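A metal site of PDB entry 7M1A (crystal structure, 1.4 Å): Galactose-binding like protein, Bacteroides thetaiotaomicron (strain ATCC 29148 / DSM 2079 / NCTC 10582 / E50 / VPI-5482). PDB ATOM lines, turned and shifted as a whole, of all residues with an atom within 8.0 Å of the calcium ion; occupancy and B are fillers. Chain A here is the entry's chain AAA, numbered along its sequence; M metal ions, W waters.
The side-chain hydroxyl of Thr 171 sits at hydrogen-bond distance from the backbone carbonyl oxygen of Val 43 (2.7 Å). OE2 of Glu 172 lies within hydrogen-bond range of N of Gly 32, at 2.8 Å. The side-chain carboxylate of Glu 172 is in salt-bridge range of the side-chain amino group of Lys 5, 2.7 Å away. The side-chain amide nitrogen (ND2) of Asn 31 sits at hydrogen-bond distance from the backbone carbonyl oxygen (O) of Gly 41, at 3.2 Å. The guanidinium group of Arg 33 is in hydrogen-bond range of the backbone carbonyl oxygen of Gly 41. The backbone NH (N) of Trp 74 sits at hydrogen-bond distance from the backbone carbonyl oxygen (O) of Glu 172 (2.9 Å). The side-chain hydroxyl of Thr 171 sits at hydrogen-bond distance from the backbone NH of Ser 35, at 2.9 Å. ND2 of Asn 31 is in hydrogen-bond range of O of Gly 42.
Five residues have an atom within 4 Å of the calcium ion: Tyr 28, Asn 31, Arg 33, Thr 171 and Glu 172. The nearest printed residue that does not touch the calcium ion is Val 29 (4.02 Å).
The calcium ion is bound by the backbone carbonyl oxygen of Tyr 28 (2.3 Å), the backbone carbonyl oxygen of Thr 171 (2.3 Å), the side-chain carboxylate of Glu 172 (2.3 Å), the backbone carbonyl oxygen of Arg 33 (2.4 Å), water W1 (2.4 Å) and the side-chain amide oxygen of Asn 31 (2.4 Å). The calcium ion has six donor atoms within binding distance.
Water W1 lies within hydrogen-bond range of OG of Ser 35 (2.7 Å), O of Gly 42 (2.8 Å), O of Val 43 (3.2 Å), OG1 of Thr 171 (3.2 Å) and ND2 of Asn 31 (3.4 Å).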
ATOM      1  N   LYS A   5      32.136  19.490  20.128  1.00  0.00           N
ATOM      2  CA  LYS A   5      32.083  20.876  19.622  1.00  0.00           C
ATOM      3  C   LYS A   5      33.436  21.591  19.692  1.00  0.00           C
ATOM      4  O   LYS A   5      33.625  22.555  18.938  1.00  0.00           O
ATOM      5  CB  LYS A   5      31.030  21.716  20.369  1.00  0.00           C
ATOM      6  CG  LYS A   5      29.629  21.229  20.092  1.00  0.00           C
ATOM      7  CD  LYS A   5      28.600  21.927  20.965  1.00  0.00           C
ATOM      8  CE  LYS A   5      27.184  21.586  20.531  1.00  0.00           C
ATOM      9  NZ  LYS A   5      26.181  22.218  21.419  1.00  0.00           N
ATOM     10  N   LYS A  25      29.251  35.880  16.676  1.00  0.00           N
ATOM     11  CA  LYS A  25      30.374  35.130  16.105  1.00  0.00           C
ATOM     12  C   LYS A  25      29.889  33.700  15.940  1.00  0.00           C
ATOM     13  O   LYS A  25      29.111  33.149  16.715  1.00  0.00           O
ATOM     14  CB  LYS A  25      31.570  35.060  17.100  1.00  0.00           C
ATOM     15  CG  LYS A  25      32.837  34.735  16.334  1.00  0.00           C
ATOM     16  CD  LYS A  25      33.391  35.865  15.492  1.00  0.00           C
ATOM     17  CE  LYS A  25      34.595  35.326  14.671  1.00  0.00           C
ATOM     18  NZ  LYS A  25      34.316  34.111  13.816  1.00  0.00           N
ATOM     19  N   MET A  26      30.305  33.067  14.832  1.00  0.00           N
ATOM     20  CA  MET A  26      29.810  31.751  14.518  1.00  0.00           C
ATOM     21  C   MET A  26      30.124  30.786  15.679  1.00  0.00           C
ATOM     22  O   MET A  26      29.307  29.925  16.005  1.00  0.00           O
ATOM     23  CB  MET A  26      30.351  31.197  13.182  1.00  0.00           C
ATOM     24  CG  MET A  26      29.445  29.965  12.769  1.00  0.00           C
ATOM     25  SD  MET A  26      30.087  29.130  11.117  1.00  0.00           S
ATOM     26  CE  MET A  26      29.880  30.697   9.900  1.00  0.00           C
ATOM     27  N   GLU A  27      31.362  30.903  16.273  1.00  0.00           N
ATOM     28  CA  GLU A  27      31.773  29.953  17.293  1.00  0.00           C
ATOM     29  C   GLU A  27      30.835  30.013  18.499  1.00  0.00           C
ATOM     30  O   GLU A  27      30.828  29.092  19.282  1.00  0.00           O
ATOM     31  CB  GLU A  27      33.200  30.320  17.753  1.00  0.00           C
ATOM     32  CG  GLU A  27      34.327  30.009  16.731  1.00  0.00           C
ATOM     33  CD  GLU A  27      34.532  30.981  15.614  1.00  0.00           C
ATOM     34  OE1 GLU A  27      33.814  32.008  15.456  1.00  0.00           O
ATOM     35  OE2 GLU A  27      35.570  30.743  14.891  1.00  0.00           O
ATOM     36  N   TYR A  28      30.068  31.106  18.640  1.00  0.00           N
ATOM     37  CA  TYR A  28      29.158  31.155  19.776  1.00  0.00           C
ATOM     38  C   TYR A  28      27.977  30.184  19.684  1.00  0.00           C
ATOM     39  O   TYR A  28      27.293  30.007  20.729  1.00  0.00           O
ATOM     40  CB  TYR A  28      28.657  32.611  19.957  1.00  0.00           C
ATOM     41  CG  TYR A  28      29.729  33.647  20.273  1.00  0.00           C
ATOM     42  CD1 TYR A  28      30.980  33.301  20.777  1.00  0.00           C
ATOM     43  CD2 TYR A  28      29.480  34.994  20.019  1.00  0.00           C
ATOM     44  CE1 TYR A  28      31.925  34.292  21.025  1.00  0.00           C
ATOM     45  CE2 TYR A  28      30.387  36.013  20.323  1.00  0.00           C
ATOM     46  CZ  TYR A  28      31.584  35.637  20.882  1.00  0.00           C
ATOM     47  OH  TYR A  28      32.534  36.598  21.066  1.00  0.00           O
ATOM     48  N   VAL A  29      27.727  29.619  18.468  1.00  0.00           N
ATOM     49  CA  VAL A  29      26.606  28.670  18.371  1.00  0.00           C
ATOM     50  C   VAL A  29      27.095  27.230  18.587  1.00  0.00           C
ATOM     51  O   VAL A  29      26.298  26.324  18.502  1.00  0.00           O
ATOM     52  CB  VAL A  29      25.777  28.821  17.098  1.00  0.00           C
ATOM     53  CG1 VAL A  29      25.242  30.245  16.970  1.00  0.00           C
ATOM     54  CG2 VAL A  29      26.471  28.322  15.826  1.00  0.00           C
ATOM     55  N   TRP A  30      28.390  27.007  18.954  1.00  0.00           N
ATOM     56  CA  TRP A  30      28.836  25.710  19.443  1.00  0.00           C
ATOM     57  C   TRP A  30      29.691  25.835  20.702  1.00  0.00           C
ATOM     58  O   TRP A  30      30.555  25.009  20.915  1.00  0.00           O
ATOM     59  CB  TRP A  30      29.467  24.868  18.304  1.00  0.00           C
ATOM     60  CG  TRP A  30      30.664  25.528  17.678  1.00  0.00           C
ATOM     61  CD1 TRP A  30      31.914  25.618  18.200  1.00  0.00           C
ATOM     62  CD2 TRP A  30      30.719  26.021  16.315  1.00  0.00           C
ATOM     63  NE1 TRP A  30      32.768  26.208  17.265  1.00  0.00           N
ATOM     64  CE2 TRP A  30      32.080  26.441  16.078  1.00  0.00           C
ATOM     65  CE3 TRP A  30      29.773  26.129  15.260  1.00  0.00           C
ATOM     66  CZ2 TRP A  30      32.509  26.963  14.877  1.00  0.00           C
ATOM     67  CZ3 TRP A  30      30.237  26.620  14.062  1.00  0.00           C
ATOM     68  CH2 TRP A  30      31.561  26.995  13.863  1.00  0.00           C
ATOM     69  N   ASN A  31      29.371  26.833  21.532  1.00  0.00           N
ATOM     70  CA  ASN A  31      30.061  27.014  22.795  1.00  0.00           C
ATOM     71  C   ASN A  31      29.438  26.242  23.944  1.00  0.00           C
ATOM     72  O   ASN A  31      29.933  26.406  25.041  1.00  0.00           O
ATOM     73  CB  ASN A  31      30.312  28.519  23.033  1.00  0.00           C
ATOM     74  CG  ASN A  31      29.023  29.263  23.375  1.00  0.00           C
ATOM     75  OD1 ASN A  31      27.935  28.666  23.394  1.00  0.00           O
ATOM     76  ND2 ASN A  31      29.109  30.591  23.502  1.00  0.00           N
ATOM     77  N   GLY A  32      28.398  25.440  23.716  1.00  0.00           N
ATOM     78  CA  GLY A  32      27.754  24.638  24.785  1.00  0.00           C
ATOM     79  C   GLY A  32      26.799  25.459  25.638  1.00  0.00           C
ATOM     80  O   GLY A  32      26.363  24.914  26.683  1.00  0.00           O
ATOM     81  N   ARG A  33      26.622  26.758  25.274  1.00  0.00           N
ATOM     82  CA  ARG A  33      25.744  27.585  26.106  1.00  0.00           C
ATOM     83  C   ARG A  33      24.533  27.978  25.275  1.00  0.00           C
ATOM     84  O   ARG A  33      24.618  28.397  24.119  1.00  0.00           O
ATOM     85  CB  ARG A  33      26.449  28.860  26.631  1.00  0.00           C
ATOM     86  CG  ARG A  33      27.574  28.488  27.569  1.00  0.00           C
ATOM     87  CD  ARG A  33      28.099  29.740  28.264  1.00  0.00           C
ATOM     88  NE  ARG A  33      29.106  30.226  27.208  1.00  0.00           N
ATOM     89  CZ  ARG A  33      30.450  29.916  27.090  1.00  0.00           C
ATOM     90  NH1 ARG A  33      30.990  28.876  27.712  1.00  0.00           N
ATOM     91  NH2 ARG A  33      31.206  30.630  26.229  1.00  0.00           N
ATOM     92  N   ILE A  34      23.343  27.843  25.896  1.00  0.00           N
ATOM     93  CA  ILE A  34      22.103  28.235  25.264  1.00  0.00           C
ATOM     94  C   ILE A  34      21.723  29.542  25.972  1.00  0.00           C
ATOM     95  O   ILE A  34      21.342  29.538  27.169  1.00  0.00           O
ATOM     96  CB  ILE A  34      21.014  27.148  25.422  1.00  0.00           C
ATOM     97  CG1 ILE A  34      21.393  25.895  24.618  1.00  0.00           C
ATOM     98  CG2 ILE A  34      19.641  27.663  25.000  1.00  0.00           C
ATOM     99  CD1 ILE A  34      20.677  24.655  25.136  1.00  0.00           C
ATOM    100  N   SER A  35      21.932  30.673  25.284  1.00  0.00           N
ATOM    101  CA  SER A  35      22.048  31.990  25.925  1.00  0.00           C
ATOM    102  C   SER A  35      20.903  32.916  25.553  1.00  0.00           C
ATOM    103  O   SER A  35      20.168  32.653  24.570  1.00  0.00           O
ATOM    104  CB  SER A  35      23.371  32.683  25.606  1.00  0.00           C
ATOM    105  OG  SER A  35      24.444  31.806  25.821  1.00  0.00           O
ATOM    106  N   GLY A  41      29.872  35.608  27.581  1.00  0.00           N
ATOM    107  CA  GLY A  41      30.482  34.439  26.933  1.00  0.00           C
ATOM    108  C   GLY A  41      30.038  34.251  25.476  1.00  0.00           C
ATOM    109  O   GLY A  41      30.365  33.169  24.908  1.00  0.00           O
ATOM    110  N   GLY A  42      29.415  35.293  24.825  1.00  0.00           N
ATOM    111  CA  GLY A  42      29.073  35.217  23.387  1.00  0.00           C
ATOM    112  C   GLY A  42      27.679  34.584  23.262  1.00  0.00           C
ATOM    113  O   GLY A  42      27.492  33.419  23.581  1.00  0.00           O
ATOM    114  N   VAL A  43      26.722  35.398  22.828  1.00  0.00           N
ATOM    115  CA  VAL A  43      25.310  34.982  22.815  1.00  0.00           C
ATOM    116  C   VAL A  43      24.913  34.119  21.628  1.00  0.00           C
ATOM    117  O   VAL A  43      24.069  33.227  21.759  1.00  0.00           O
ATOM    118  CB  VAL A  43      24.411  36.251  22.926  1.00  0.00           C
ATOM    119  CG1 VAL A  43      22.931  35.981  22.722  1.00  0.00           C
ATOM    120  CG2 VAL A  43      24.686  36.973  24.279  1.00  0.00           C
ATOM    121  N   GLY A  44      25.477  34.413  20.460  1.00  0.00           N
ATOM    122  CA  GLY A  44      25.046  33.643  19.310  1.00  0.00           C
ATOM    123  C   GLY A  44      25.635  34.255  18.039  1.00  0.00           C
ATOM    124  O   GLY A  44      26.627  35.008  18.092  1.00  0.00           O
ATOM    125  N   LEU A  45      25.036  33.925  16.885  1.00  0.00           N
ATOM    126  CA  LEU A  45      25.394  34.538  15.648  1.00  0.00           C
ATOM    127  C   LEU A  45      24.214  35.336  15.139  1.00  0.00           C
ATOM    128  O   LEU A  45      23.043  35.101  15.554  1.00  0.00           O
ATOM    129  CB  LEU A  45      25.941  33.539  14.611  1.00  0.00           C
ATOM    130  CG  LEU A  45      24.945  32.509  14.030  1.00  0.00           C
ATOM    131  CD1 LEU A  45      23.986  33.101  12.984  1.00  0.00           C
ATOM    132  CD2 LEU A  45      25.735  31.362  13.370  1.00  0.00           C
ATOM    133  N   TRP A  74      18.644  26.132  18.918  1.00  0.00           N
ATOM    134  CA  TRP A  74      17.929  26.986  19.884  1.00  0.00           C
ATOM    135  C   TRP A  74      18.001  28.439  19.402  1.00  0.00           C
ATOM    136  O   TRP A  74      19.084  28.960  19.179  1.00  0.00           O
ATOM    137  CB  TRP A  74      18.567  26.914  21.308  1.00  0.00           C
ATOM    138  CG  TRP A  74      18.333  25.582  21.933  1.00  0.00           C
ATOM    139  CD1 TRP A  74      17.361  25.301  22.842  1.00  0.00           C
ATOM    140  CD2 TRP A  74      19.037  24.317  21.698  1.00  0.00           C
ATOM    141  NE1 TRP A  74      17.435  23.976  23.218  1.00  0.00           N
ATOM    142  CE2 TRP A  74      18.488  23.349  22.559  1.00  0.00           C
ATOM    143  CE3 TRP A  74      20.178  23.915  21.003  1.00  0.00           C
ATOM    144  CZ2 TRP A  74      18.918  22.037  22.670  1.00  0.00           C
ATOM    145  CZ3 TRP A  74      20.663  22.622  21.082  1.00  0.00           C
ATOM    146  CH2 TRP A  74      20.007  21.669  21.889  1.00  0.00           C
ATOM    147  N   PHE A 170      20.595  33.051  16.162  1.00  0.00           N
ATOM    148  CA  PHE A 170      20.265  31.981  17.090  1.00  0.00           C
ATOM    149  C   PHE A 170      21.442  31.798  18.059  1.00  0.00           C
ATOM    150  O   PHE A 170      22.521  32.403  17.817  1.00  0.00           O
ATOM    151  CB  PHE A 170      19.847  30.651  16.446  1.00  0.00           C
ATOM    152  CG  PHE A 170      20.923  29.959  15.701  1.00  0.00           C
ATOM    153  CD1 PHE A 170      21.284  30.403  14.402  1.00  0.00           C
ATOM    154  CD2 PHE A 170      21.579  28.855  16.213  1.00  0.00           C
ATOM    155  CE1 PHE A 170      22.266  29.731  13.650  1.00  0.00           C
ATOM    156  CE2 PHE A 170      22.575  28.187  15.458  1.00  0.00           C
ATOM    157  CZ  PHE A 170      22.916  28.666  14.204  1.00  0.00           C
ATOM    158  N   THR A 171      21.257  30.983  19.140  1.00  0.00           N
ATOM    159  CA  THR A 171      22.264  30.908  20.183  1.00  0.00           C
ATOM    160  C   THR A 171      23.097  29.614  20.157  1.00  0.00           C
ATOM    161  O   THR A 171      24.274  29.678  20.650  1.00  0.00           O
ATOM    162  CB  THR A 171      21.677  31.126  21.590  1.00  0.00           C
ATOM    163  OG1 THR A 171      22.728  31.078  22.558  1.00  0.00           O
ATOM    164  CG2 THR A 171      20.653  30.062  22.001  1.00  0.00           C
ATOM    165  N   GLU A 172      22.575  28.459  19.729  1.00  0.00           N
ATOM    166  CA  GLU A 172      23.329  27.211  19.858  1.00  0.00           C
ATOM    167  C   GLU A 172      22.736  26.190  18.896  1.00  0.00           C
ATOM    168  O   GLU A 172      21.512  26.205  18.658  1.00  0.00           O
ATOM    169  CB  GLU A 172      23.245  26.632  21.304  1.00  0.00           C
ATOM    170  CG  GLU A 172      24.196  25.487  21.608  1.00  0.00           C
ATOM    171  CD  GLU A 172      25.686  25.847  21.596  1.00  0.00           C
ATOM    172  OE1 GLU A 172      26.036  27.037  21.570  1.00  0.00           O
ATOM    173  OE2 GLU A 172      26.486  24.913  21.720  1.00  0.00           O
ATOM    174  N   LEU A 173      23.597  25.292  18.388  1.00  0.00           N
ATOM    175  CA  LEU A 173      23.115  24.098  17.711  1.00  0.00           C
ATOM    176  C   LEU A 173      23.873  22.914  18.281  1.00  0.00           C
ATOM    177  O   LEU A 173      24.916  23.098  18.935  1.00  0.00           O
ATOM    178  CB  LEU A 173      23.179  24.223  16.181  1.00  0.00           C
ATOM    179  CG  LEU A 173      24.474  24.769  15.567  1.00  0.00           C
ATOM    180  CD1 LEU A 173      25.592  23.759  15.768  1.00  0.00           C
ATOM    181  CD2 LEU A 173      24.218  25.065  14.091  1.00  0.00           C
HETATM  182 CA    CA M   1      25.827  29.225  22.280  1.00  0.00          CA
HETATM  183  O   HOH W   1      25.793  31.197  23.562  1.00  0.00           O
